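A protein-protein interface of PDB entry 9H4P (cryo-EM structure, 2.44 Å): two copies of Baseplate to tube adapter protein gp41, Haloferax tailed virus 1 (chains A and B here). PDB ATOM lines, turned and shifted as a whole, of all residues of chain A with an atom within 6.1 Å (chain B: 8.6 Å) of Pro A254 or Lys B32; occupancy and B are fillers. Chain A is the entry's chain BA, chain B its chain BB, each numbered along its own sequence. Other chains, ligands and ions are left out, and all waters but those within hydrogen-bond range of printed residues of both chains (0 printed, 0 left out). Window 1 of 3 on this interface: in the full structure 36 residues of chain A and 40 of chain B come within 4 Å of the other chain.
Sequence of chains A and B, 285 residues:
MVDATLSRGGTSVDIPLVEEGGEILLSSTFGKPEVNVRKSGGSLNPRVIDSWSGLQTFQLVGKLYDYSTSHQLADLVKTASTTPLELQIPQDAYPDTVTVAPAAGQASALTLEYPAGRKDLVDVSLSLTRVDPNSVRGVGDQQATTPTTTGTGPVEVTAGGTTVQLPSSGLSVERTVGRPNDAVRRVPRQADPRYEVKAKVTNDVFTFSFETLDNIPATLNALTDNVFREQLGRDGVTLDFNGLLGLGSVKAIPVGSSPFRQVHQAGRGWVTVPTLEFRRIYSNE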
ATOM      1  N   VAL A 227     -15.309  -3.459 -25.606  1.00  0.00           N
ATOM      2  CA  VAL A 227     -16.150  -2.567 -26.402  1.00  0.00           C
ATOM      3  C   VAL A 227     -17.639  -2.820 -26.123  1.00  0.00           C
ATOM      4  O   VAL A 227     -18.373  -1.862 -25.879  1.00  0.00           O
ATOM      5  CB  VAL A 227     -15.805  -2.602 -27.911  1.00  0.00           C
ATOM      6  CG1 VAL A 227     -16.674  -1.660 -28.736  1.00  0.00           C
ATOM      7  CG2 VAL A 227     -14.328  -2.317 -28.177  1.00  0.00           C
ATOM      8  N   PHE A 228     -18.069  -4.095 -26.133  1.00  0.00           N
ATOM      9  CA  PHE A 228     -19.489  -4.435 -26.165  1.00  0.00           C
ATOM     10  C   PHE A 228     -20.084  -4.725 -24.782  1.00  0.00           C
ATOM     11  O   PHE A 228     -21.296  -4.580 -24.609  1.00  0.00           O
ATOM     12  CB  PHE A 228     -19.767  -5.527 -27.206  1.00  0.00           C
ATOM     13  CG  PHE A 228     -19.715  -5.002 -28.619  1.00  0.00           C
ATOM     14  CD1 PHE A 228     -20.783  -4.276 -29.136  1.00  0.00           C
ATOM     15  CD2 PHE A 228     -18.587  -5.182 -29.413  1.00  0.00           C
ATOM     16  CE1 PHE A 228     -20.738  -3.762 -30.424  1.00  0.00           C
ATOM     17  CE2 PHE A 228     -18.543  -4.668 -30.703  1.00  0.00           C
ATOM     18  CZ  PHE A 228     -19.616  -3.960 -31.204  1.00  0.00           C
ATOM     19  N   ARG A 229     -19.244  -5.107 -23.804  1.00  0.00           N
ATOM     20  CA  ARG A 229     -19.732  -5.494 -22.482  1.00  0.00           C
ATOM     21  C   ARG A 229     -19.478  -4.414 -21.425  1.00  0.00           C
ATOM     22  O   ARG A 229     -20.209  -4.353 -20.435  1.00  0.00           O
ATOM     23  CB  ARG A 229     -19.259  -6.900 -22.098  1.00  0.00           C
ATOM     24  CG  ARG A 229     -19.754  -7.975 -23.056  1.00  0.00           C
ATOM     25  CD  ARG A 229     -19.618  -9.388 -22.525  1.00  0.00           C
ATOM     26  NE  ARG A 229     -20.701  -9.737 -21.610  1.00  0.00           N
ATOM     27  CZ  ARG A 229     -20.560 -10.171 -20.356  1.00  0.00           C
ATOM     28  NH1 ARG A 229     -21.631 -10.457 -19.635  1.00  0.00           N
ATOM     29  NH2 ARG A 229     -19.359 -10.338 -19.828  1.00  0.00           N
ATOM     30  N   GLU A 230     -18.461  -3.563 -21.637  1.00  0.00           N
ATOM     31  CA  GLU A 230     -18.243  -2.384 -20.805  1.00  0.00           C
ATOM     32  C   GLU A 230     -19.176  -1.256 -21.256  1.00  0.00           C
ATOM     33  O   GLU A 230     -19.555  -1.207 -22.427  1.00  0.00           O
ATOM     34  CB  GLU A 230     -16.789  -1.911 -20.914  1.00  0.00           C
ATOM     35  CG  GLU A 230     -15.789  -2.820 -20.224  1.00  0.00           C
ATOM     36  CD  GLU A 230     -16.004  -2.973 -18.731  1.00  0.00           C
ATOM     37  OE1 GLU A 230     -15.872  -1.973 -18.010  1.00  0.00           O
ATOM     38  OE2 GLU A 230     -16.320  -4.091 -18.296  1.00  0.00           O
ATOM     39  N   GLN A 231     -19.538  -0.350 -20.329  1.00  0.00           N
ATOM     40  CA  GLN A 231     -20.187   0.913 -20.665  1.00  0.00           C
ATOM     41  C   GLN A 231     -19.105   1.943 -20.995  1.00  0.00           C
ATOM     42  O   GLN A 231     -18.199   2.164 -20.190  1.00  0.00           O
ATOM     43  CB  GLN A 231     -21.040   1.432 -19.500  1.00  0.00           C
ATOM     44  CG  GLN A 231     -22.396   0.747 -19.359  1.00  0.00           C
ATOM     45  CD  GLN A 231     -22.324  -0.618 -18.718  1.00  0.00           C
ATOM     46  OE1 GLN A 231     -21.551  -0.858 -17.792  1.00  0.00           O
ATOM     47  NE2 GLN A 231     -23.156  -1.529 -19.200  1.00  0.00           N
ATOM     48  N   LEU A 232     -19.218   2.590 -22.166  1.00  0.00           N
ATOM     49  CA  LEU A 232     -18.145   3.426 -22.696  1.00  0.00           C
ATOM     50  C   LEU A 232     -18.251   4.888 -22.243  1.00  0.00           C
ATOM     51  O   LEU A 232     -17.309   5.648 -22.465  1.00  0.00           O
ATOM     52  CB  LEU A 232     -18.065   3.290 -24.226  1.00  0.00           C
ATOM     53  CG  LEU A 232     -17.713   1.901 -24.770  1.00  0.00           C
ATOM     54  CD1 LEU A 232     -17.788   1.870 -26.292  1.00  0.00           C
ATOM     55  CD2 LEU A 232     -16.340   1.430 -24.298  1.00  0.00           C
ATOM     56  N   VAL A 237     -14.589   4.106 -28.547  1.00  0.00           N
ATOM     57  CA  VAL A 237     -13.453   3.442 -29.163  1.00  0.00           C
ATOM     58  C   VAL A 237     -12.579   4.503 -29.835  1.00  0.00           C
ATOM     59  O   VAL A 237     -13.100   5.408 -30.487  1.00  0.00           O
ATOM     60  CB  VAL A 237     -13.949   2.375 -30.165  1.00  0.00           C
ATOM     61  CG1 VAL A 237     -12.971   2.070 -31.293  1.00  0.00           C
ATOM     62  CG2 VAL A 237     -14.369   1.088 -29.477  1.00  0.00           C
ATOM     63  N   ALA A 252     -14.854   6.832 -32.228  1.00  0.00           N
ATOM     64  CA  ALA A 252     -16.039   6.206 -32.807  1.00  0.00           C
ATOM     65  C   ALA A 252     -16.738   5.308 -31.782  1.00  0.00           C
ATOM     66  O   ALA A 252     -16.168   5.023 -30.727  1.00  0.00           O
ATOM     67  CB  ALA A 252     -15.648   5.433 -34.049  1.00  0.00           C
ATOM     68  N   ILE A 253     -17.967   4.859 -32.099  1.00  0.00           N
ATOM     69  CA  ILE A 253     -18.722   3.952 -31.236  1.00  0.00           C
ATOM     70  C   ILE A 253     -19.581   3.005 -32.088  1.00  0.00           C
ATOM     71  O   ILE A 253     -20.067   3.407 -33.149  1.00  0.00           O
ATOM     72  CB  ILE A 253     -19.540   4.722 -30.161  1.00  0.00           C
ATOM     73  CG1 ILE A 253     -19.896   3.846 -28.949  1.00  0.00           C
ATOM     74  CG2 ILE A 253     -20.767   5.423 -30.754  1.00  0.00           C
ATOM     75  CD1 ILE A 253     -20.277   4.612 -27.688  1.00  0.00           C
ATOM     76  N   PRO A 254     -19.772   1.715 -31.688  1.00  0.00           N
ATOM     77  CA  PRO A 254     -20.843   0.883 -32.255  1.00  0.00           C
ATOM     78  C   PRO A 254     -22.230   1.379 -31.841  1.00  0.00           C
ATOM     79  O   PRO A 254     -22.407   1.854 -30.716  1.00  0.00           O
ATOM     80  CB  PRO A 254     -20.595  -0.518 -31.664  1.00  0.00           C
ATOM     81  CG  PRO A 254     -19.160  -0.480 -31.171  1.00  0.00           C
ATOM     82  CD  PRO A 254     -18.926   0.956 -30.746  1.00  0.00           C
ATOM     83  N   VAL A 255     -23.210   1.266 -32.757  1.00  0.00           N
ATOM     84  CA  VAL A 255     -24.549   1.819 -32.565  1.00  0.00           C
ATOM     85  C   VAL A 255     -25.600   0.777 -32.961  1.00  0.00           C
ATOM     86  O   VAL A 255     -25.462   0.126 -33.996  1.00  0.00           O
ATOM     87  CB  VAL A 255     -24.755   3.132 -33.361  1.00  0.00           C
ATOM     88  CG1 VAL A 255     -26.113   3.776 -33.099  1.00  0.00           C
ATOM     89  CG2 VAL A 255     -23.644   4.156 -33.151  1.00  0.00           C
ATOM     90  N   GLY A 256     -26.657   0.639 -32.142  1.00  0.00           N
ATOM     91  CA  GLY A 256     -27.854  -0.099 -32.526  1.00  0.00           C
ATOM     92  C   GLY A 256     -27.766  -1.599 -32.242  1.00  0.00           C
ATOM     93  O   GLY A 256     -26.885  -2.037 -31.505  1.00  0.00           O
ATOM     94  N   SER A 257     -28.683  -2.371 -32.852  1.00  0.00           N
ATOM     95  CA  SER A 257     -28.998  -3.736 -32.446  1.00  0.00           C
ATOM     96  C   SER A 257     -28.040  -4.788 -33.021  1.00  0.00           C
ATOM     97  O   SER A 257     -27.981  -5.896 -32.485  1.00  0.00           O
ATOM     98  CB  SER A 257     -30.438  -4.083 -32.761  1.00  0.00           C
ATOM     99  OG  SER A 257     -31.330  -3.175 -32.135  1.00  0.00           O
ATOM    100  N   SER A 258     -27.310  -4.467 -34.109  1.00  0.00           N
ATOM    101  CA  SER A 258     -26.490  -5.460 -34.805  1.00  0.00           C
ATOM    102  C   SER A 258     -25.191  -4.902 -35.415  1.00  0.00           C
ATOM    103  O   SER A 258     -24.836  -5.295 -36.530  1.00  0.00           O
ATOM    104  CB  SER A 258     -27.314  -6.221 -35.831  1.00  0.00           C
ATOM    105  OG  SER A 258     -27.760  -5.361 -36.870  1.00  0.00           O
ATOM    106  N   PRO A 259     -24.412  -4.020 -34.720  1.00  0.00           N
ATOM    107  CA  PRO A 259     -23.148  -3.506 -35.264  1.00  0.00           C
ATOM    108  C   PRO A 259     -21.993  -4.510 -35.330  1.00  0.00           C
ATOM    109  O   PRO A 259     -21.004  -4.237 -36.009  1.00  0.00           O
ATOM    110  CB  PRO A 259     -22.787  -2.335 -34.325  1.00  0.00           C
ATOM    111  CG  PRO A 259     -23.420  -2.713 -32.999  1.00  0.00           C
ATOM    112  CD  PRO A 259     -24.696  -3.428 -33.396  1.00  0.00           C
ATOM    113  N   LEU A 276     -18.494  -5.237 -38.744  1.00  0.00           N
ATOM    114  CA  LEU A 276     -18.183  -4.520 -37.518  1.00  0.00           C
ATOM    115  C   LEU A 276     -18.312  -3.028 -37.835  1.00  0.00           C
ATOM    116  O   LEU A 276     -17.483  -2.477 -38.563  1.00  0.00           O
ATOM    117  CB  LEU A 276     -16.769  -4.912 -37.053  1.00  0.00           C
ATOM    118  CG  LEU A 276     -16.153  -4.083 -35.919  1.00  0.00           C
ATOM    119  CD1 LEU A 276     -16.960  -4.179 -34.625  1.00  0.00           C
ATOM    120  CD2 LEU A 276     -14.702  -4.485 -35.674  1.00  0.00           C
ATOM    121  N   GLU A 277     -19.379  -2.392 -37.323  1.00  0.00           N
ATOM    122  CA  GLU A 277     -19.728  -1.018 -37.670  1.00  0.00           C
ATOM    123  C   GLU A 277     -19.375  -0.063 -36.526  1.00  0.00           C
ATOM    124  O   GLU A 277     -19.707  -0.327 -35.368  1.00  0.00           O
ATOM    125  CB  GLU A 277     -21.229  -0.889 -37.957  1.00  0.00           C
ATOM    126  CG  GLU A 277     -21.709  -1.612 -39.205  1.00  0.00           C
ATOM    127  CD  GLU A 277     -23.180  -1.403 -39.509  1.00  0.00           C
ATOM    128  OE1 GLU A 277     -23.694  -0.301 -39.251  1.00  0.00           O
ATOM    129  OE2 GLU A 277     -23.807  -2.347 -40.000  1.00  0.00           O
ATOM    130  N   PHE A 278     -18.743   1.066 -36.884  1.00  0.00           N
ATOM    131  CA  PHE A 278     -18.480   2.168 -35.967  1.00  0.00           C
ATOM    132  C   PHE A 278     -18.945   3.485 -36.595  1.00  0.00           C
ATOM    133  O   PHE A 278     -18.650   3.751 -37.760  1.00  0.00           O
ATOM    134  CB  PHE A 278     -16.977   2.285 -35.686  1.00  0.00           C
ATOM    135  CG  PHE A 278     -16.311   1.115 -34.999  1.00  0.00           C
ATOM    136  CD1 PHE A 278     -16.409   0.958 -33.619  1.00  0.00           C
ATOM    137  CD2 PHE A 278     -15.542   0.204 -35.718  1.00  0.00           C
ATOM    138  CE1 PHE A 278     -15.779  -0.102 -32.976  1.00  0.00           C
ATOM    139  CE2 PHE A 278     -14.909  -0.852 -35.072  1.00  0.00           C
ATOM    140  CZ  PHE A 278     -15.033  -1.006 -33.705  1.00  0.00           C
ATOM    141  N   ARG A 279     -19.658   4.306 -35.812  1.00  0.00           N
ATOM    142  CA  ARG A 279     -19.980   5.668 -36.218  1.00  0.00           C
ATOM    143  C   ARG A 279     -18.989   6.632 -35.561  1.00  0.00           C
ATOM    144  O   ARG A 279     -18.775   6.552 -34.351  1.00  0.00           O
ATOM    145  CB  ARG A 279     -21.422   6.022 -35.835  1.00  0.00           C
ATOM    146  CG  ARG A 279     -21.837   7.413 -36.295  1.00  0.00           C
ATOM    147  CD  ARG A 279     -23.312   7.727 -36.148  1.00  0.00           C
ATOM    148  NE  ARG A 279     -23.570   9.091 -36.597  1.00  0.00           N
ATOM    149  CZ  ARG A 279     -24.769   9.655 -36.714  1.00  0.00           C
ATOM    150  NH1 ARG A 279     -24.874  10.907 -37.131  1.00  0.00           N
ATOM    151  NH2 ARG A 279     -25.862   8.978 -36.413  1.00  0.00           N
ATOM    152  N   THR B  29     -24.708 -12.148 -32.204  1.00  0.00           N
ATOM    153  CA  THR B  29     -24.690 -10.718 -32.489  1.00  0.00           C
ATOM    154  C   THR B  29     -24.528  -9.940 -31.185  1.00  0.00           C
ATOM    155  O   THR B  29     -25.028 -10.357 -30.139  1.00  0.00           O
ATOM    156  CB  THR B  29     -25.934 -10.250 -33.262  1.00  0.00           C
ATOM    157  OG1 THR B  29     -27.022 -10.067 -32.354  1.00  0.00           O
ATOM    158  CG2 THR B  29     -26.363 -11.194 -34.366  1.00  0.00           C
ATOM    159  N   PHE B  30     -23.825  -8.806 -31.280  1.00  0.00           N
ATOM    160  CA  PHE B  30     -23.602  -7.904 -30.162  1.00  0.00           C
ATOM    161  C   PHE B  30     -24.064  -6.515 -30.580  1.00  0.00           C
ATOM    162  O   PHE B  30     -23.868  -6.118 -31.729  1.00  0.00           O
ATOM    163  CB  PHE B  30     -22.112  -7.844 -29.809  1.00  0.00           C
ATOM    164  CG  PHE B  30     -21.510  -9.146 -29.340  1.00  0.00           C
ATOM    165  CD1 PHE B  30     -21.215 -10.163 -30.244  1.00  0.00           C
ATOM    166  CD2 PHE B  30     -21.222  -9.347 -27.995  1.00  0.00           C
ATOM    167  CE1 PHE B  30     -20.658 -11.357 -29.810  1.00  0.00           C
ATOM    168  CE2 PHE B  30     -20.662 -10.541 -27.562  1.00  0.00           C
ATOM    169  CZ  PHE B  30     -20.379 -11.542 -28.471  1.00  0.00           C
ATOM    170  N   GLY B  31     -24.669  -5.789 -29.637  1.00  0.00           N
ATOM    171  CA  GLY B  31     -25.171  -4.469 -29.959  1.00  0.00           C
ATOM    172  C   GLY B  31     -25.348  -3.589 -28.730  1.00  0.00           C
ATOM    173  O   GLY B  31     -25.354  -4.068 -27.594  1.00  0.00           O
ATOM    174  N   LYS B  32     -25.501  -2.291 -29.009  1.00  0.00           N
ATOM    175  CA  LYS B  32     -25.805  -1.283 -28.010  1.00  0.00           C
ATOM    176  C   LYS B  32     -27.119  -0.613 -28.402  1.00  0.00           C
ATOM    177  O   LYS B  32     -27.108   0.475 -28.983  1.00  0.00           O
ATOM    178  CB  LYS B  32     -24.644  -0.290 -27.887  1.00  0.00           C
ATOM    179  CG  LYS B  32     -23.374  -0.871 -27.281  1.00  0.00           C
ATOM    180  CD  LYS B  32     -22.250   0.132 -27.159  1.00  0.00           C
ATOM    181  CE  LYS B  32     -20.970  -0.471 -26.617  1.00  0.00           C
ATOM    182  NZ  LYS B  32     -21.040  -0.736 -25.160  1.00  0.00           N
ATOM    183  N   PRO B  33     -28.291  -1.252 -28.133  1.00  0.00           N
ATOM    184  CA  PRO B  33     -29.582  -0.632 -28.443  1.00  0.00           C
ATOM    185  C   PRO B  33     -29.879   0.604 -27.591  1.00  0.00           C
ATOM    186  O   PRO B  33     -30.770   1.379 -27.940  1.00  0.00           O
ATOM    187  CB  PRO B  33     -30.616  -1.745 -28.187  1.00  0.00           C
ATOM    188  CG  PRO B  33     -29.932  -2.682 -27.209  1.00  0.00           C
ATOM    189  CD  PRO B  33     -28.455  -2.595 -27.541  1.00  0.00           C
ATOM    190  N   GLU B  34     -29.106   0.797 -26.503  1.00  0.00           N
ATOM    191  CA  GLU B  34     -29.357   1.831 -25.504  1.00  0.00           C
ATOM    192  C   GLU B  34     -28.306   2.953 -25.516  1.00  0.00           C
ATOM    193  O   GLU B  34     -28.279   3.745 -24.570  1.00  0.00           O
ATOM    194  CB  GLU B  34     -29.508   1.224 -24.100  1.00  0.00           C
ATOM    195  CG  GLU B  34     -30.645   0.220 -23.954  1.00  0.00           C
ATOM    196  CD  GLU B  34     -32.035   0.716 -24.309  1.00  0.00           C
ATOM    197  OE1 GLU B  34     -32.378   1.847 -23.923  1.00  0.00           O
ATOM    198  OE2 GLU B  34     -32.768  -0.028 -24.978  1.00  0.00           O
ATOM    199  N   VAL B  35     -27.456   3.056 -26.560  1.00  0.00           N
ATOM    200  CA  VAL B  35     -26.653   4.269 -26.732  1.00  0.00           C
ATOM    201  C   VAL B  35     -27.562   5.394 -27.222  1.00  0.00           C
ATOM    202  O   VAL B  35     -28.399   5.184 -28.102  1.00  0.00           O
ATOM    203  CB  VAL B  35     -25.426   4.138 -27.666  1.00  0.00           C
ATOM    204  CG1 VAL B  35     -24.227   3.491 -26.991  1.00  0.00           C
ATOM    205  CG2 VAL B  35     -25.727   3.477 -29.008  1.00  0.00           C
ATOM    206  N   ASN B  36     -27.357   6.592 -26.663  1.00  0.00           N
ATOM    207  CA  ASN B  36     -27.995   7.792 -27.176  1.00  0.00           C
ATOM    208  C   ASN B  36     -27.006   8.568 -28.048  1.00  0.00           C
ATOM    209  O   ASN B  36     -26.276   9.426 -27.548  1.00  0.00           O
ATOM    210  CB  ASN B  36     -28.607   8.628 -26.047  1.00  0.00           C
ATOM    211  CG  ASN B  36     -29.767   7.929 -25.366  1.00  0.00           C
ATOM    212  OD1 ASN B  36     -30.823   7.737 -25.966  1.00  0.00           O
ATOM    213  ND2 ASN B  36     -29.596   7.561 -24.106  1.00  0.00           N
ATOM    214  N   VAL B  37     -26.990   8.249 -29.352  1.00  0.00           N
ATOM    215  CA  VAL B  37     -26.329   9.075 -30.356  1.00  0.00           C
ATOM    216  C   VAL B  37     -27.264  10.246 -30.663  1.00  0.00           C
ATOM    217  O   VAL B  37     -28.405  10.027 -31.075  1.00  0.00           O
ATOM    218  CB  VAL B  37     -25.989   8.270 -31.634  1.00  0.00           C
ATOM    219  CG1 VAL B  37     -25.300   9.122 -32.695  1.00  0.00           C
ATOM    220  CG2 VAL B  37     -25.161   7.025 -31.336  1.00  0.00           C
ATOM    221  N   VAL B  48     -22.310  11.390 -27.851  1.00  0.00           N
ATOM    222  CA  VAL B  48     -22.917  10.102 -27.537  1.00  0.00           C
ATOM    223  C   VAL B  48     -22.859   9.861 -26.024  1.00  0.00           C
ATOM    224  O   VAL B  48     -22.099  10.521 -25.314  1.00  0.00           O
ATOM    225  CB  VAL B  48     -22.253   8.940 -28.314  1.00  0.00           C
ATOM    226  CG1 VAL B  48     -22.359   9.085 -29.829  1.00  0.00           C
ATOM    227  CG2 VAL B  48     -20.812   8.660 -27.887  1.00  0.00           C
ATOM    228  N   ILE B  49     -23.666   8.896 -25.553  1.00  0.00           N
ATOM    229  CA  ILE B  49     -23.605   8.395 -24.185  1.00  0.00           C
ATOM    230  C   ILE B  49     -23.993   6.914 -24.172  1.00  0.00           C
ATOM    231  O   ILE B  49     -25.062   6.537 -24.657  1.00  0.00           O
ATOM    232  CB  ILE B  49     -24.425   9.268 -23.193  1.00  0.00           C
ATOM    233  CG1 ILE B  49     -24.532   8.662 -21.785  1.00  0.00           C
ATOM    234  CG2 ILE B  49     -25.806   9.620 -23.741  1.00  0.00           C
ATOM    235  CD1 ILE B  49     -23.270   8.712 -20.939  1.00  0.00           C
ATOM    236  N   ASP B  50     -23.089   6.085 -23.627  1.00  0.00           N
ATOM    237  CA  ASP B  50     -23.300   4.664 -23.390  1.00  0.00           C
ATOM    238  C   ASP B  50     -23.368   4.428 -21.879  1.00  0.00           C
ATOM    239  O   ASP B  50     -22.403   4.711 -21.167  1.00  0.00           O
ATOM    240  CB  ASP B  50     -22.165   3.850 -24.017  1.00  0.00           C
ATOM    241  CG  ASP B  50     -22.302   2.349 -23.839  1.00  0.00           C
ATOM    242  OD1 ASP B  50     -23.433   1.873 -23.614  1.00  0.00           O
ATOM    243  OD2 ASP B  50     -21.274   1.662 -23.937  1.00  0.00           O
ATOM    244  N   SER B  51     -24.505   3.902 -21.393  1.00  0.00           N
ATOM    245  CA  SER B  51     -24.832   4.025 -19.976  1.00  0.00           C
ATOM    246  C   SER B  51     -25.753   2.908 -19.468  1.00  0.00           C
ATOM    247  O   SER B  51     -26.408   3.074 -18.434  1.00  0.00           O
ATOM    248  CB  SER B  51     -25.417   5.400 -19.708  1.00  0.00           C
ATOM    249  OG  SER B  51     -25.567   5.631 -18.315  1.00  0.00           O
ATOM    250  N   TRP B  52     -25.786   1.769 -20.182  1.00  0.00           N
ATOM    251  CA  TRP B  52     -26.720   0.676 -19.930  1.00  0.00           C
ATOM    252  C   TRP B  52     -26.099  -0.654 -20.366  1.00  0.00           C
ATOM    253  O   TRP B  52     -25.073  -0.668 -21.047  1.00  0.00           O
ATOM    254  CB  TRP B  52     -28.039   0.925 -20.685  1.00  0.00           C
ATOM    255  CG  TRP B  52     -28.833   2.128 -20.264  1.00  0.00           C
ATOM    256  CD1 TRP B  52     -28.841   3.354 -20.869  1.00  0.00           C
ATOM    257  CD2 TRP B  52     -29.760   2.224 -19.161  1.00  0.00           C
ATOM    258  NE1 TRP B  52     -29.703   4.200 -20.220  1.00  0.00           N
ATOM    259  CE2 TRP B  52     -30.289   3.537 -19.169  1.00  0.00           C
ATOM    260  CE3 TRP B  52     -30.212   1.333 -18.175  1.00  0.00           C
ATOM    261  CZ2 TRP B  52     -31.239   3.967 -18.232  1.00  0.00           C
ATOM    262  CZ3 TRP B  52     -31.148   1.757 -17.251  1.00  0.00           C
ATOM    263  CH2 TRP B  52     -31.657   3.060 -17.279  1.00  0.00           C
ATOM    264  N   SER B  53     -26.742  -1.768 -19.979  1.00  0.00           N
ATOM    265  CA  SER B  53     -26.428  -3.105 -20.476  1.00  0.00           C
ATOM    266  C   SER B  53     -26.547  -3.168 -22.006  1.00  0.00           C
ATOM    267  O   SER B  53     -27.333  -2.426 -22.598  1.00  0.00           O
ATOM    268  CB  SER B  53     -27.324  -4.130 -19.811  1.00  0.00           C
ATOM    269  OG  SER B  53     -28.698  -3.791 -19.966  1.00  0.00           O
ATOM    270  N   GLY B  54     -25.768  -4.066 -22.633  1.00  0.00           N
ATOM    271  CA  GLY B  54     -25.800  -4.280 -24.075  1.00  0.00           C
ATOM    272  C   GLY B  54     -26.619  -5.513 -24.459  1.00  0.00           C
ATOM    273  O   GLY B  54     -27.016  -6.290 -23.589  1.00  0.00           O
ATOM    274  N   LEU B  55     -26.869  -5.671 -25.768  1.00  0.00           N
ATOM    275  CA  LEU B  55     -27.458  -6.890 -26.305  1.00  0.00           C
ATOM    276  C   LEU B  55     -26.365  -7.910 -26.613  1.00  0.00           C
ATOM    277  O   LEU B  55     -25.288  -7.556 -27.096  1.00  0.00           O
ATOM    278  CB  LEU B  55     -28.253  -6.573 -27.579  1.00  0.00           C
ATOM    279  CG  LEU B  55     -29.777  -6.682 -27.476  1.00  0.00           C
ATOM    280  CD1 LEU B  55     -30.455  -6.100 -28.704  1.00  0.00           C
ATOM    281  CD2 LEU B  55     -30.225  -8.123 -27.257  1.00  0.00           C
ATOM    282  N   GLN B  56     -26.673  -9.183 -26.339  1.00  0.00           N
ATOM    283  CA  GLN B  56     -26.062 -10.291 -27.058  1.00  0.00           C
ATOM    284  C   GLN B  56     -27.154 -11.288 -27.444  1.00  0.00           C
ATOM    285  O   GLN B  56     -27.993 -11.644 -26.614  1.00  0.00           O
ATOM    286  CB  GLN B  56     -24.929 -10.943 -26.259  1.00  0.00           C
ATOM    287  CG  GLN B  56     -24.191 -12.025 -27.045  1.00  0.00           C
ATOM    288  CD  GLN B  56     -23.009 -12.638 -26.334  1.00  0.00           C
ATOM    289  OE1 GLN B  56     -22.680 -12.298 -25.197  1.00  0.00           O
ATOM    290  NE2 GLN B  56     -22.341 -13.555 -27.016  1.00  0.00           N
ATOM    291  N   ALA B 191     -23.410  -5.897 -17.585  1.00  0.00           N
ATOM    292  CA  ALA B 191     -23.113  -6.059 -19.003  1.00  0.00           C
ATOM    293  C   ALA B 191     -24.353  -6.559 -19.754  1.00  0.00           C
ATOM    294  O   ALA B 191     -24.650  -6.088 -20.854  1.00  0.00           O
ATOM    295  CB  ALA B 191     -21.931  -6.981 -19.189  1.00  0.00           C
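Printed residues of chain B within 4 Å of Gln A231: Asp B50, Ser B51, Trp B52 and Ser B53. Ala A252 touches none of the printed residues of chain B. Ile A253 touches none of the printed residues of chain B. Of chain B, only Lys B32 comes within 4 Å of Pro A254. Of the printed residues of chain B, Gly A256 touches Gly B31, Lys B32 and Pro B33. Of chain A, only Val A227 (3.0 Å), Phe A228 (3.9 Å), Glu A230 (3.1 Å), Leu A232 (3.96 Å), Pro A254 (3.96 Å) and Gly A256 (2.9 Å) come within 4 Å of Lys B32. Printed residues of chain A within 4 Å of Pro B33: Gly A256 (3.7 Å). Printed residues of chain A within 4 Å of Val B37: Val A255 (3.7 Å) and Arg A279 (3.8 Å). Of the printed residues of chain A, Ser B51 touches Gln A231. Of the printed residues of chain A, Ala B191 touches Arg A229. The nearest residue of chain A that does not touch Lys B32 is Val A255 (4.3 Å).
The backbone carbonyl oxygen (O) of Ile A253 lies within hydrogen-bond range of the backbone NH (N) of Arg A279 (2.8 Å). O of Pro A259 is in hydrogen-bond range of N of Glu A277 (2.8 Å). O of Gly B31 is in hydrogen-bond range of N of Leu B55, at 2.9 Å. The side-chain carboxylate (OD2) of Asp B50 lies within salt-bridge range of the side-chain amino group (NZ) of Lys B32, 2.7 Å away. The backbone NH (N) of Gly B54 is in hydrogen-bond range of the backbone carbonyl oxygen (O) of Ala B191 (2.9 Å).
O of Gly A256 sits at hydrogen-bond distance from N of Lys B32, 2.9 Å away. N of Leu A232 is in hydrogen-bond range of OD2 of Asp B50 (2.9 Å). NE2 of Gln A231 lies within hydrogen-bond range of O of Trp B52 (2.8 Å). The backbone carbonyl oxygen (O) of Glu A230 lies within hydrogen-bond range of the side-chain amino group (NZ) of Lys B32, 3.1 Å away. The backbone carbonyl oxygen (O) of Val A227 lies within hydrogen-bond range of the side-chain amino group (NZ) of Lys B32 (3.0 Å).
No position is printed for both chains. Of the 20 pairs that touch across the chains among the printed residues, none has its exchanged pair printed and touching as well.
Among the printed residues, merely in contact across the chains: Phe A228 with Phe B30 (3.9 Å), Phe A228 with Lys B32 (3.9 Å), Arg A229 with Ala B191 (3.4 Å), Glu A230 with Asp B50 (3.7 Å), Gln A231 with Asp B50 (3.5 Å), Gln A231 with Ser B51 (3.99 Å), Gln A231 with Ser B53 (3.7 Å), Leu A232 with Lys B32 (3.96 Å), Pro A254 with Lys B32 (3.96 Å), Val A255 with Val B37 (3.7 Å), Gly A256 with Gly B31 (3.4 Å), Gly A256 with Pro B33 (3.7 Å), Pro A259 with Phe B30 (3.3 Å), Pro A259 with Gly B31 (3.6 Å) and Arg A279 with Val B37 (3.8 Å).
Of the 19 printed residues of chain A, 11 touch a printed residue of chain B. Printed residues of chain B that touch a printed residue of chain A: Phe B30, Gly B31, Lys B32, Pro B33, Val B37, Asp B50, Ser B51, Trp B52, Ser B53 and Ala B191. Hydrophobic or aromatic side chains of chain B within 4 Å of the printed part of chain A: Phe B30, Val B37 and Ala B191.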
